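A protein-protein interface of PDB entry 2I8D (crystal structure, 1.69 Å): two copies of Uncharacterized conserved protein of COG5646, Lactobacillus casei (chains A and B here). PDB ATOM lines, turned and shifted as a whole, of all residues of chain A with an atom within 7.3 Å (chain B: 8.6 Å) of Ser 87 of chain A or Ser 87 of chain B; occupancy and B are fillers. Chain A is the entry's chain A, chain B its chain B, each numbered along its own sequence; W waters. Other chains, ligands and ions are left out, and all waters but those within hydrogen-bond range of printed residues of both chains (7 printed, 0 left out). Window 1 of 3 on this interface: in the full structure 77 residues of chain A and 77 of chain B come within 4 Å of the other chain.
Water W5 lies within hydrogen-bond range of the side-chain amide nitrogen (NE2) of Gln 88 of chain A (2.9 Å) and the side-chain carboxylate (OE1) of Glu 68 of chain B (2.9 Å).
Ser 87 of chain B touches its own counterpart, Ser 87 of chain A. Ser 87 of chain A touches Gln 88 of chain B, and with the chains exchanged Gln 88 of chain A touches Ser 87 of chain B.
Of the printed residues of chain A, Ser 87 of chain B touches Ser 87 (3.7 Å), Gln 88 (3.3 Å), Ile 89 (2.8 Å) and Arg 91 (3.4 Å). Of chain B, only Val 65 (3.1 Å), Ala 66 (3.9 Å), Met 72 (3.5 Å), His 86 (3.1 Å) and Ser 87 (2.8 Å) come within 4 Å of Ile 89 of chain A. The nearest printed residue of chain A that does not touch Ile 76 of chain B is Ile 90 of chain A (7.3 Å).
The backbone carbonyl oxygen (O) of Gly 55 of chain B is in hydrogen-bond range of the backbone NH (N) of Ala 66 of chain B, 2.9 Å away.
Of the 23 printed residues of chain B, 18 touch a printed residue of chain A. Hydrophobic or aromatic side chains of chain B within 4 Å of the printed part of chain A: His 62, Ile 67, Pro 69, Met 72, Ile 76, Ile 79, Tyr 84, His 86, Ile 89 and Ile 90. Printed residues of chain A that touch a printed residue of chain B: Val 65, Ala 66, Ile 67, Pro 69, Met 72, Asp 85, His 86, Ser 87, Gln 88, Ile 89, Ile 90 and Arg 91. Along chain A the printed residues that touch a printed residue of chain B span positions 65 to 91. Among the printed residues, Asp or Glu carboxylates within 4 Å of a Lys or Arg side-chain nitrogen of the other chain: Asp 85 of chain A with Arg 91 of chain B.
N of Arg 91 of chain A lies within hydrogen-bond range of O of Asp 85 of chain B (2.9 Å). NE2 of Gln 88 of chain B lies close to N of Pro 69 of chain A, 3.5 Å away. The backbone carbonyl oxygen (O) of Ile 67 of chain A is in hydrogen-bond range of the side-chain amide nitrogen (NE2) of Gln 88 of chain B. The backbone carbonyl oxygen of Ser 87 of chain A sits at hydrogen-bond distance from the backbone NH of Ile 89 of chain B (2.8 Å). The backbone NH (N) of Ser 87 of chain B is in hydrogen-bond range of the backbone carbonyl oxygen (O) of Ile 89 of chain A (2.8 Å). The side-chain amide nitrogen of Gln 88 of chain A sits close to the backbone nitrogen of Pro 69 of chain B, 3.5 Å away. N of Ile 90 of chain A is in hydrogen-bond range of O of Val 65 of chain B (2.8 Å). N of Ile 67 of chain B lies within hydrogen-bond range of O of Gln 88 of chain A. N of Ile 90 of chain B is in hydrogen-bond range of O of Val 65 of chain A, 2.9 Å away. The side-chain carboxylate (OD2) of Asp 85 of chain A lies within salt-bridge range of the guanidinium group (NH2) of Arg 91 of chain B (3.3 Å).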
ATOM      1  N   GLN A  43       8.859  -4.232 -12.462  1.00  0.00           N
ATOM      2  CA  GLN A  43       8.111  -5.371 -12.975  1.00  0.00           C
ATOM      3  C   GLN A  43       6.795  -5.545 -12.219  1.00  0.00           C
ATOM      4  O   GLN A  43       6.687  -5.191 -11.022  1.00  0.00           O
ATOM      5  CB  GLN A  43       8.925  -6.671 -12.916  1.00  0.00           C
ATOM      6  CG  GLN A  43       9.045  -7.292 -11.537  1.00  0.00           C
ATOM      7  CD  GLN A  43       9.886  -8.572 -11.513  1.00  0.00           C
ATOM      8  OE1 GLN A  43       9.499  -9.614 -12.054  1.00  0.00           O
ATOM      9  NE2 GLN A  43      11.034  -8.499 -10.844  1.00  0.00           N
ATOM     10  N   VAL A  65       8.612 -16.352 -15.045  1.00  0.00           N
ATOM     11  CA  VAL A  65       7.778 -16.296 -13.833  1.00  0.00           C
ATOM     12  C   VAL A  65       8.631 -16.533 -12.590  1.00  0.00           C
ATOM     13  O   VAL A  65       9.230 -17.589 -12.436  1.00  0.00           O
ATOM     14  CB  VAL A  65       6.658 -17.322 -13.903  1.00  0.00           C
ATOM     15  CG1 VAL A  65       5.879 -17.390 -12.575  1.00  0.00           C
ATOM     16  CG2 VAL A  65       5.737 -16.973 -15.090  1.00  0.00           C
ATOM     17  N   ALA A  66       8.637 -15.520 -11.724  1.00  0.00           N
ATOM     18  CA  ALA A  66       9.510 -15.450 -10.546  1.00  0.00           C
ATOM     19  C   ALA A  66       8.741 -15.929  -9.346  1.00  0.00           C
ATOM     20  O   ALA A  66       7.602 -15.450  -9.074  1.00  0.00           O
ATOM     21  CB  ALA A  66      10.036 -14.030 -10.306  1.00  0.00           C
ATOM     22  N   ILE A  67       9.341 -16.877  -8.626  1.00  0.00           N
ATOM     23  CA  ILE A  67       8.740 -17.490  -7.456  1.00  0.00           C
ATOM     24  C   ILE A  67       9.771 -17.536  -6.306  1.00  0.00           C
ATOM     25  O   ILE A  67      10.982 -17.312  -6.518  1.00  0.00           O
ATOM     26  CB  ILE A  67       8.215 -18.903  -7.763  1.00  0.00           C
ATOM     27  CG1 ILE A  67       9.340 -19.799  -8.311  1.00  0.00           C
ATOM     28  CG2 ILE A  67       7.016 -18.830  -8.767  1.00  0.00           C
ATOM     29  CD1 ILE A  67       8.945 -21.264  -8.460  1.00  0.00           C
ATOM     30  N   PRO A  69      12.082 -19.025  -3.139  1.00  0.00           N
ATOM     31  CA  PRO A  69      12.969 -20.201  -3.089  1.00  0.00           C
ATOM     32  C   PRO A  69      12.263 -21.478  -2.614  1.00  0.00           C
ATOM     33  O   PRO A  69      12.462 -22.554  -3.180  1.00  0.00           O
ATOM     34  CB  PRO A  69      14.054 -19.766  -2.074  1.00  0.00           C
ATOM     35  CG  PRO A  69      14.104 -18.281  -2.246  1.00  0.00           C
ATOM     36  CD  PRO A  69      12.668 -17.865  -2.445  1.00  0.00           C
ATOM     37  N   MET A  72      10.028 -22.870  -5.366  1.00  0.00           N
ATOM     38  CA  MET A  72      10.825 -23.542  -6.393  1.00  0.00           C
ATOM     39  C   MET A  72      11.244 -24.947  -5.890  1.00  0.00           C
ATOM     40  O   MET A  72      11.064 -25.935  -6.546  1.00  0.00           O
ATOM     41  CB  MET A  72      12.069 -22.692  -6.708  1.00  0.00           C
ATOM     42  CG  MET A  72      13.015 -23.270  -7.787  1.00  0.00           C
ATOM     43  SD  MET A  72      12.137 -23.525  -9.469  1.00  0.00           S
ATOM     44  CE  MET A  72      12.379 -21.841 -10.142  1.00  0.00           C
ATOM     45  N   ASP A  85      11.997 -25.356 -18.127  1.00  0.00           N
ATOM     46  CA  ASP A  85      13.294 -25.076 -17.519  1.00  0.00           C
ATOM     47  C   ASP A  85      13.123 -24.074 -16.384  1.00  0.00           C
ATOM     48  O   ASP A  85      12.179 -23.270 -16.362  1.00  0.00           O
ATOM     49  CB  ASP A  85      14.279 -24.485 -18.534  1.00  0.00           C
ATOM     50  CG  ASP A  85      14.817 -25.517 -19.514  1.00  0.00           C
ATOM     51  OD1 ASP A  85      14.647 -26.752 -19.306  1.00  0.00           O
ATOM     52  OD2 ASP A  85      15.413 -25.069 -20.513  1.00  0.00           O
ATOM     53  N   HIS A  86      14.056 -24.112 -15.440  1.00  0.00           N
ATOM     54  CA  HIS A  86      14.000 -23.185 -14.323  1.00  0.00           C
ATOM     55  C   HIS A  86      15.432 -22.733 -14.040  1.00  0.00           C
ATOM     56  O   HIS A  86      16.377 -23.396 -14.452  1.00  0.00           O
ATOM     57  CB  HIS A  86      13.350 -23.852 -13.137  1.00  0.00           C
ATOM     58  CG  HIS A  86      14.005 -25.130 -12.725  1.00  0.00           C
ATOM     59  ND1 HIS A  86      15.069 -25.169 -11.857  1.00  0.00           N
ATOM     60  CD2 HIS A  86      13.742 -26.419 -13.065  1.00  0.00           C
ATOM     61  CE1 HIS A  86      15.421 -26.432 -11.659  1.00  0.00           C
ATOM     62  NE2 HIS A  86      14.643 -27.208 -12.393  1.00  0.00           N
ATOM     63  N   SER A  87      15.573 -21.602 -13.352  1.00  0.00           N
ATOM     64  CA  SER A  87      16.854 -21.025 -13.039  1.00  0.00           C
ATOM     65  C   SER A  87      16.812 -20.317 -11.687  1.00  0.00           C
ATOM     66  O   SER A  87      15.821 -19.669 -11.354  1.00  0.00           O
ATOM     67  CB  SER A  87      17.254 -20.044 -14.138  1.00  0.00           C
ATOM     68  OG  SER A  87      18.574 -19.597 -13.959  1.00  0.00           O
ATOM     69  N   GLN A  88      17.876 -20.477 -10.899  1.00  0.00           N
ATOM     70  CA  GLN A  88      18.023 -19.792  -9.637  1.00  0.00           C
ATOM     71  C   GLN A  88      19.380 -19.091  -9.663  1.00  0.00           C
ATOM     72  O   GLN A  88      20.422 -19.754  -9.844  1.00  0.00           O
ATOM     73  CB  GLN A  88      17.961 -20.783  -8.463  1.00  0.00           C
ATOM     74  CG  GLN A  88      16.721 -21.743  -8.504  1.00  0.00           C
ATOM     75  CD  GLN A  88      16.760 -22.839  -9.552  1.00  0.00           C
ATOM     76  OE1 GLN A  88      15.726 -23.088 -10.197  1.00  0.00           O
ATOM     77  NE2 GLN A  88      17.937 -23.499  -9.768  1.00  0.00           N
ATOM     78  N   ILE A  89      19.345 -17.770  -9.567  1.00  0.00           N
ATOM     79  CA  ILE A  89      20.535 -16.953  -9.746  1.00  0.00           C
ATOM     80  C   ILE A  89      20.683 -15.948  -8.609  1.00  0.00           C
ATOM     81  O   ILE A  89      19.676 -15.442  -8.034  1.00  0.00           O
ATOM     82  CB  ILE A  89      20.563 -16.218 -11.127  1.00  0.00           C
ATOM     83  CG1 ILE A  89      19.426 -15.212 -11.241  1.00  0.00           C
ATOM     84  CG2 ILE A  89      20.594 -17.233 -12.320  1.00  0.00           C
ATOM     85  CD1 ILE A  89      19.892 -13.764 -11.155  1.00  0.00           C
ATOM     86  N   ILE A  90      21.945 -15.671  -8.287  1.00  0.00           N
ATOM     87  CA  ILE A  90      22.343 -14.547  -7.460  1.00  0.00           C
ATOM     88  C   ILE A  90      22.929 -13.465  -8.340  1.00  0.00           C
ATOM     89  O   ILE A  90      23.760 -13.762  -9.238  1.00  0.00           O
ATOM     90  CB  ILE A  90      23.382 -14.932  -6.398  1.00  0.00           C
ATOM     91  CG1 ILE A  90      22.900 -16.124  -5.594  1.00  0.00           C
ATOM     92  CG2 ILE A  90      23.771 -13.732  -5.487  1.00  0.00           C
ATOM     93  CD1 ILE A  90      24.029 -16.839  -4.799  1.00  0.00           C
ATOM     94  N   ARG A  91      22.494 -12.230  -8.118  1.00  0.00           N
ATOM     95  CA  ARG A  91      22.986 -11.093  -8.910  1.00  0.00           C
ATOM     96  C   ARG A  91      24.155 -10.452  -8.198  1.00  0.00           C
ATOM     97  O   ARG A  91      24.009  -9.937  -7.076  1.00  0.00           O
ATOM     98  CB  ARG A  91      21.897 -10.027  -9.132  1.00  0.00           C
ATOM     99  CG  ARG A  91      20.806 -10.474 -10.045  1.00  0.00           C
ATOM    100  CD  ARG A  91      19.657  -9.480 -10.060  1.00  0.00           C
ATOM    101  NE  ARG A  91      18.527 -10.058 -10.783  1.00  0.00           N
ATOM    102  CZ  ARG A  91      17.309 -10.255 -10.282  1.00  0.00           C
ATOM    103  NH1 ARG A  91      16.981  -9.855  -9.056  1.00  0.00           N
ATOM    104  NH2 ARG A  91      16.382 -10.812 -11.055  1.00  0.00           N
ATOM    105  N   GLN B  43      26.414 -21.093 -22.242  1.00  0.00           N
ATOM    106  CA  GLN B  43      27.014 -20.448 -21.118  1.00  0.00           C
ATOM    107  C   GLN B  43      28.088 -21.317 -20.449  1.00  0.00           C
ATOM    108  O   GLN B  43      28.051 -22.545 -20.555  1.00  0.00           O
ATOM    109  CB  GLN B  43      25.960 -20.056 -20.069  1.00  0.00           C
ATOM    110  CG  GLN B  43      25.397 -21.200 -19.280  1.00  0.00           C
ATOM    111  CD  GLN B  43      24.360 -20.733 -18.250  1.00  0.00           C
ATOM    112  OE1 GLN B  43      24.647 -19.945 -17.340  1.00  0.00           O
ATOM    113  NE2 GLN B  43      23.149 -21.221 -18.399  1.00  0.00           N
ATOM    114  N   PHE B  52      26.081 -30.793 -12.765  1.00  0.00           N
ATOM    115  CA  PHE B  52      26.098 -29.327 -12.672  1.00  0.00           C
ATOM    116  C   PHE B  52      26.436 -28.872 -11.256  1.00  0.00           C
ATOM    117  O   PHE B  52      25.868 -29.373 -10.282  1.00  0.00           O
ATOM    118  CB  PHE B  52      24.725 -28.766 -13.082  1.00  0.00           C
ATOM    119  CG  PHE B  52      24.584 -27.284 -12.918  1.00  0.00           C
ATOM    120  CD1 PHE B  52      25.013 -26.417 -13.912  1.00  0.00           C
ATOM    121  CD2 PHE B  52      24.041 -26.743 -11.763  1.00  0.00           C
ATOM    122  CE1 PHE B  52      24.883 -25.059 -13.748  1.00  0.00           C
ATOM    123  CE2 PHE B  52      23.898 -25.386 -11.623  1.00  0.00           C
ATOM    124  CZ  PHE B  52      24.333 -24.552 -12.608  1.00  0.00           C
ATOM    125  N   GLY B  55      26.599 -22.090 -12.802  1.00  0.00           N
ATOM    126  CA  GLY B  55      26.593 -21.417 -14.125  1.00  0.00           C
ATOM    127  C   GLY B  55      26.828 -19.916 -14.043  1.00  0.00           C
ATOM    128  O   GLY B  55      26.735 -19.309 -12.960  1.00  0.00           O
ATOM    129  N   ASN B  57      26.503 -15.969 -16.289  1.00  0.00           N
ATOM    130  CA  ASN B  57      26.040 -15.162 -17.427  1.00  0.00           C
ATOM    131  C   ASN B  57      26.150 -13.688 -17.086  1.00  0.00           C
ATOM    132  O   ASN B  57      25.745 -13.263 -16.002  1.00  0.00           O
ATOM    133  CB  ASN B  57      24.612 -15.529 -17.800  1.00  0.00           C
ATOM    134  CG  ASN B  57      24.521 -16.386 -19.079  1.00  0.00           C
ATOM    135  OD1 ASN B  57      25.377 -16.321 -19.980  1.00  0.00           O
ATOM    136  ND2 ASN B  57      23.478 -17.195 -19.153  1.00  0.00           N
ATOM    137  N   HIS B  62      25.105  -6.741 -13.894  1.00  0.00           N
ATOM    138  CA  HIS B  62      25.628  -7.754 -12.985  1.00  0.00           C
ATOM    139  C   HIS B  62      26.138  -9.003 -13.684  1.00  0.00           C
ATOM    140  O   HIS B  62      25.848  -9.247 -14.867  1.00  0.00           O
ATOM    141  CB  HIS B  62      24.536  -8.177 -11.994  1.00  0.00           C
ATOM    142  CG  HIS B  62      23.315  -8.741 -12.658  1.00  0.00           C
ATOM    143  ND1 HIS B  62      22.125  -8.050 -12.750  1.00  0.00           N
ATOM    144  CD2 HIS B  62      23.096  -9.944 -13.245  1.00  0.00           C
ATOM    145  CE1 HIS B  62      21.224  -8.807 -13.365  1.00  0.00           C
ATOM    146  NE2 HIS B  62      21.788  -9.963 -13.672  1.00  0.00           N
ATOM    147  N   ALA B  64      25.385 -12.865 -13.260  1.00  0.00           N
ATOM    148  CA  ALA B  64      24.369 -13.800 -12.733  1.00  0.00           C
ATOM    149  C   ALA B  64      25.065 -15.102 -12.458  1.00  0.00           C
ATOM    150  O   ALA B  64      25.674 -15.670 -13.368  1.00  0.00           O
ATOM    151  CB  ALA B  64      23.196 -14.011 -13.730  1.00  0.00           C
ATOM    152  N   VAL B  65      25.053 -15.538 -11.206  1.00  0.00           N
ATOM    153  CA  VAL B  65      25.581 -16.844 -10.787  1.00  0.00           C
ATOM    154  C   VAL B  65      24.390 -17.797 -10.524  1.00  0.00           C
ATOM    155  O   VAL B  65      23.571 -17.549  -9.636  1.00  0.00           O
ATOM    156  CB  VAL B  65      26.521 -16.678  -9.527  1.00  0.00           C
ATOM    157  CG1 VAL B  65      26.960 -18.009  -8.868  1.00  0.00           C
ATOM    158  CG2 VAL B  65      27.782 -15.815  -9.931  1.00  0.00           C
ATOM    159  N   ALA B  66      24.370 -18.854 -11.316  1.00  0.00           N
ATOM    160  CA  ALA B  66      23.304 -19.855 -11.357  1.00  0.00           C
ATOM    161  C   ALA B  66      23.702 -21.010 -10.436  1.00  0.00           C
ATOM    162  O   ALA B  66      24.839 -21.572 -10.508  1.00  0.00           O
ATOM    163  CB  ALA B  66      23.092 -20.353 -12.773  1.00  0.00           C
ATOM    164  N   ILE B  67      22.784 -21.381  -9.556  1.00  0.00           N
ATOM    165  CA  ILE B  67      23.016 -22.428  -8.590  1.00  0.00           C
ATOM    166  C   ILE B  67      21.784 -23.325  -8.527  1.00  0.00           C
ATOM    167  O   ILE B  67      20.716 -22.973  -9.051  1.00  0.00           O
ATOM    168  CB  ILE B  67      23.343 -21.876  -7.161  1.00  0.00           C
ATOM    169  CG1 ILE B  67      22.208 -20.982  -6.633  1.00  0.00           C
ATOM    170  CG2 ILE B  67      24.713 -21.114  -7.200  1.00  0.00           C
ATOM    171  CD1 ILE B  67      22.380 -20.453  -5.249  1.00  0.00           C
ATOM    172  N   GLU B  68      21.948 -24.487  -7.929  1.00  0.00           N
ATOM    173  CA  GLU B  68      20.848 -25.452  -7.870  1.00  0.00           C
ATOM    174  C   GLU B  68      19.787 -25.019  -6.838  1.00  0.00           C
ATOM    175  O   GLU B  68      20.096 -24.271  -5.904  1.00  0.00           O
ATOM    176  CB  GLU B  68      21.346 -26.845  -7.541  1.00  0.00           C
ATOM    177  CG  GLU B  68      22.175 -27.513  -8.660  1.00  0.00           C
ATOM    178  CD  GLU B  68      21.312 -28.063  -9.805  1.00  0.00           C
ATOM    179  OE1 GLU B  68      20.335 -27.392 -10.215  1.00  0.00           O
ATOM    180  OE2 GLU B  68      21.654 -29.160 -10.322  1.00  0.00           O
ATOM    181  N   PRO B  69      18.530 -25.516  -7.000  1.00  0.00           N
ATOM    182  CA  PRO B  69      17.468 -25.130  -6.046  1.00  0.00           C
ATOM    183  C   PRO B  69      17.788 -25.404  -4.579  1.00  0.00           C
ATOM    184  O   PRO B  69      17.505 -24.560  -3.725  1.00  0.00           O
ATOM    185  CB  PRO B  69      16.258 -25.961  -6.510  1.00  0.00           C
ATOM    186  CG  PRO B  69      16.550 -26.282  -7.969  1.00  0.00           C
ATOM    187  CD  PRO B  69      18.017 -26.422  -8.059  1.00  0.00           C
ATOM    188  N   MET B  72      20.273 -22.794  -3.381  1.00  0.00           N
ATOM    189  CA  MET B  72      19.614 -21.476  -3.165  1.00  0.00           C
ATOM    190  C   MET B  72      18.825 -21.477  -1.826  1.00  0.00           C
ATOM    191  O   MET B  72      19.026 -20.653  -0.932  1.00  0.00           O
ATOM    192  CB  MET B  72      18.631 -21.185  -4.287  1.00  0.00           C
ATOM    193  CG  MET B  72      17.905 -19.899  -4.091  1.00  0.00           C
ATOM    194  SD  MET B  72      19.102 -18.343  -4.116  1.00  0.00           S
ATOM    195  CE  MET B  72      19.223 -18.242  -6.070  1.00  0.00           C
ATOM    196  N   ILE B  76      19.848 -18.913   1.508  1.00  0.00           N
ATOM    197  CA  ILE B  76      19.113 -17.614   1.530  1.00  0.00           C
ATOM    198  C   ILE B  76      19.585 -16.676   2.654  1.00  0.00           C
ATOM    199  O   ILE B  76      19.909 -15.498   2.406  1.00  0.00           O
ATOM    200  CB  ILE B  76      17.598 -17.797   1.580  1.00  0.00           C
ATOM    201  CG1 ILE B  76      17.096 -18.471   0.293  1.00  0.00           C
ATOM    202  CG2 ILE B  76      16.884 -16.403   1.767  1.00  0.00           C
ATOM    203  CD1 ILE B  76      17.434 -17.637  -0.987  1.00  0.00           C
ATOM    204  N   ILE B  79      23.077 -15.301   1.729  1.00  0.00           N
ATOM    205  CA  ILE B  79      22.974 -14.414   0.560  1.00  0.00           C
ATOM    206  C   ILE B  79      22.437 -13.044   0.967  1.00  0.00           C
ATOM    207  O   ILE B  79      22.957 -12.020   0.555  1.00  0.00           O
ATOM    208  CB  ILE B  79      22.094 -15.085  -0.572  1.00  0.00           C
ATOM    209  CG1 ILE B  79      22.755 -16.349  -1.136  1.00  0.00           C
ATOM    210  CG2 ILE B  79      21.887 -14.070  -1.711  1.00  0.00           C
ATOM    211  CD1 ILE B  79      21.801 -17.348  -1.859  1.00  0.00           C
ATOM    212  N   TYR B  84      23.122  -9.443  -1.498  1.00  0.00           N
ATOM    213  CA  TYR B  84      22.884  -9.625  -2.905  1.00  0.00           C
ATOM    214  C   TYR B  84      21.453 -10.085  -3.104  1.00  0.00           C
ATOM    215  O   TYR B  84      20.926 -10.845  -2.304  1.00  0.00           O
ATOM    216  CB  TYR B  84      23.803 -10.683  -3.488  1.00  0.00           C
ATOM    217  CG  TYR B  84      25.281 -10.365  -3.346  1.00  0.00           C
ATOM    218  CD1 TYR B  84      25.870  -9.357  -4.122  1.00  0.00           C
ATOM    219  CD2 TYR B  84      26.080 -11.020  -2.429  1.00  0.00           C
ATOM    220  CE1 TYR B  84      27.188  -9.036  -4.019  1.00  0.00           C
ATOM    221  CE2 TYR B  84      27.446 -10.697  -2.321  1.00  0.00           C
ATOM    222  CZ  TYR B  84      27.995  -9.725  -3.125  1.00  0.00           C
ATOM    223  OH  TYR B  84      29.349  -9.401  -3.022  1.00  0.00           O
ATOM    224  N   ASP B  85      20.865  -9.618  -4.191  1.00  0.00           N
ATOM    225  CA  ASP B  85      19.553 -10.061  -4.642  1.00  0.00           C
ATOM    226  C   ASP B  85      19.649 -11.449  -5.320  1.00  0.00           C
ATOM    227  O   ASP B  85      20.685 -11.846  -5.893  1.00  0.00           O
ATOM    228  CB  ASP B  85      18.967  -9.062  -5.633  1.00  0.00           C
ATOM    229  CG  ASP B  85      18.524  -7.759  -4.979  1.00  0.00           C
ATOM    230  OD1 ASP B  85      18.522  -7.648  -3.742  1.00  0.00           O
ATOM    231  OD2 ASP B  85      18.166  -6.851  -5.753  1.00  0.00           O
ATOM    232  N   HIS B  86      18.539 -12.161  -5.302  1.00  0.00           N
ATOM    233  CA  HIS B  86      18.483 -13.501  -5.878  1.00  0.00           C
ATOM    234  C   HIS B  86      17.130 -13.642  -6.565  1.00  0.00           C
ATOM    235  O   HIS B  86      16.158 -12.921  -6.265  1.00  0.00           O
ATOM    236  CB  HIS B  86      18.710 -14.583  -4.850  1.00  0.00           C
ATOM    237  CG  HIS B  86      17.754 -14.537  -3.695  1.00  0.00           C
ATOM    238  ND1 HIS B  86      16.528 -15.162  -3.725  1.00  0.00           N
ATOM    239  CD2 HIS B  86      17.828 -13.910  -2.493  1.00  0.00           C
ATOM    240  CE1 HIS B  86      15.887 -14.926  -2.591  1.00  0.00           C
ATOM    241  NE2 HIS B  86      16.652 -14.168  -1.824  1.00  0.00           N
ATOM    242  N   SER B  87      17.107 -14.529  -7.531  1.00  0.00           N
ATOM    243  CA  SER B  87      15.894 -14.754  -8.310  1.00  0.00           C
ATOM    244  C   SER B  87      15.734 -16.213  -8.670  1.00  0.00           C
ATOM    245  O   SER B  87      16.712 -16.876  -9.022  1.00  0.00           O
ATOM    246  CB  SER B  87      15.947 -13.888  -9.589  1.00  0.00           C
ATOM    247  OG  SER B  87      14.716 -13.923 -10.229  1.00  0.00           O
ATOM    248  N   GLN B  88      14.484 -16.701  -8.632  1.00  0.00           N
ATOM    249  CA  GLN B  88      14.168 -18.065  -8.992  1.00  0.00           C
ATOM    250  C   GLN B  88      13.034 -18.004 -10.009  1.00  0.00           C
ATOM    251  O   GLN B  88      11.948 -17.444  -9.716  1.00  0.00           O
ATOM    252  CB  GLN B  88      13.753 -18.938  -7.791  1.00  0.00           C
ATOM    253  CG  GLN B  88      14.775 -18.898  -6.647  1.00  0.00           C
ATOM    254  CD  GLN B  88      14.801 -17.613  -5.882  1.00  0.00           C
ATOM    255  OE1 GLN B  88      15.890 -17.098  -5.560  1.00  0.00           O
ATOM    256  NE2 GLN B  88      13.595 -17.065  -5.550  1.00  0.00           N
ATOM    257  N   ILE B  89      13.337 -18.434 -11.240  1.00  0.00           N
ATOM    258  CA  ILE B  89      12.365 -18.286 -12.314  1.00  0.00           C
ATOM    259  C   ILE B  89      12.111 -19.578 -13.071  1.00  0.00           C
ATOM    260  O   ILE B  89      12.990 -20.444 -13.147  1.00  0.00           O
ATOM    261  CB  ILE B  89      12.742 -17.168 -13.295  1.00  0.00           C
ATOM    262  CG1 ILE B  89      14.056 -17.480 -13.997  1.00  0.00           C
ATOM    263  CG2 ILE B  89      12.759 -15.773 -12.588  1.00  0.00           C
ATOM    264  CD1 ILE B  89      13.867 -18.091 -15.372  1.00  0.00           C
ATOM    265  N   ILE B  90      10.888 -19.693 -13.586  1.00  0.00           N
ATOM    266  CA  ILE B  90      10.488 -20.701 -14.540  1.00  0.00           C
ATOM    267  C   ILE B  90      10.318 -20.016 -15.880  1.00  0.00           C
ATOM    268  O   ILE B  90       9.663 -18.975 -15.968  1.00  0.00           O
ATOM    269  CB  ILE B  90       9.137 -21.380 -14.130  1.00  0.00           C
ATOM    270  CG1 ILE B  90       9.246 -21.956 -12.724  1.00  0.00           C
ATOM    271  CG2 ILE B  90       8.718 -22.470 -15.158  1.00  0.00           C
ATOM    272  CD1 ILE B  90       7.921 -22.460 -12.150  1.00  0.00           C
ATOM    273  N   ARG B  91      10.898 -20.614 -16.925  1.00  0.00           N
ATOM    274  CA  ARG B  91      10.799 -20.067 -18.281  1.00  0.00           C
ATOM    275  C   ARG B  91       9.622 -20.731 -19.004  1.00  0.00           C
ATOM    276  O   ARG B  91       9.591 -21.956 -19.158  1.00  0.00           O
ATOM    277  CB  ARG B  91      12.107 -20.287 -19.059  1.00  0.00           C
ATOM    278  CG  ARG B  91      13.280 -19.417 -18.563  1.00  0.00           C
ATOM    279  CD  ARG B  91      14.488 -19.461 -19.493  1.00  0.00           C
ATOM    280  NE  ARG B  91      15.146 -20.767 -19.558  1.00  0.00           N
ATOM    281  CZ  ARG B  91      16.179 -21.168 -18.816  1.00  0.00           C
ATOM    282  NH1 ARG B  91      16.710 -20.394 -17.877  1.00  0.00           N
ATOM    283  NH2 ARG B  91      16.684 -22.381 -19.013  1.00  0.00           N
ATOM    284  N   TRP B 121       9.678 -10.379   1.375  1.00  0.00           N
ATOM    285  CA  TRP B 121      10.356 -11.521   0.768  1.00  0.00           C
ATOM    286  C   TRP B 121      10.614 -12.624   1.769  1.00  0.00           C
ATOM    287  O   TRP B 121      10.844 -12.370   2.967  1.00  0.00           O
ATOM    288  CB  TRP B 121      11.733 -11.108   0.244  1.00  0.00           C
ATOM    289  CG  TRP B 121      11.769 -10.035  -0.768  1.00  0.00           C
ATOM    290  CD1 TRP B 121      12.230  -8.769  -0.593  1.00  0.00           C
ATOM    291  CD2 TRP B 121      11.400 -10.153  -2.143  1.00  0.00           C
ATOM    292  NE1 TRP B 121      12.151  -8.069  -1.772  1.00  0.00           N
ATOM    293  CE2 TRP B 121      11.615  -8.884  -2.737  1.00  0.00           C
ATOM    294  CE3 TRP B 121      10.865 -11.191  -2.928  1.00  0.00           C
ATOM    295  CZ2 TRP B 121      11.359  -8.643  -4.080  1.00  0.00           C
ATOM    296  CZ3 TRP B 121      10.605 -10.948  -4.265  1.00  0.00           C
ATOM    297  CH2 TRP B 121      10.842  -9.682  -4.828  1.00  0.00           C
HETATM  298  O   HOH W   1      15.608 -13.087 -12.799  1.00  0.00           O
HETATM  299  O   HOH W   2      22.419  -8.037  -6.031  1.00  0.00           O
HETATM  300  O   HOH W   3      11.175 -23.711 -20.493  1.00  0.00           O
HETATM  301  O   HOH W   4      20.139 -22.430 -11.815  1.00  0.00           O
HETATM  302  O   HOH W   5      19.073 -25.253 -11.774  1.00  0.00           O
HETATM  303  O   HOH W   6      15.177 -22.694  -4.732  1.00  0.00           O
HETATM  304  O   HOH W   7      12.278 -14.958  -7.489  1.00  0.00           O
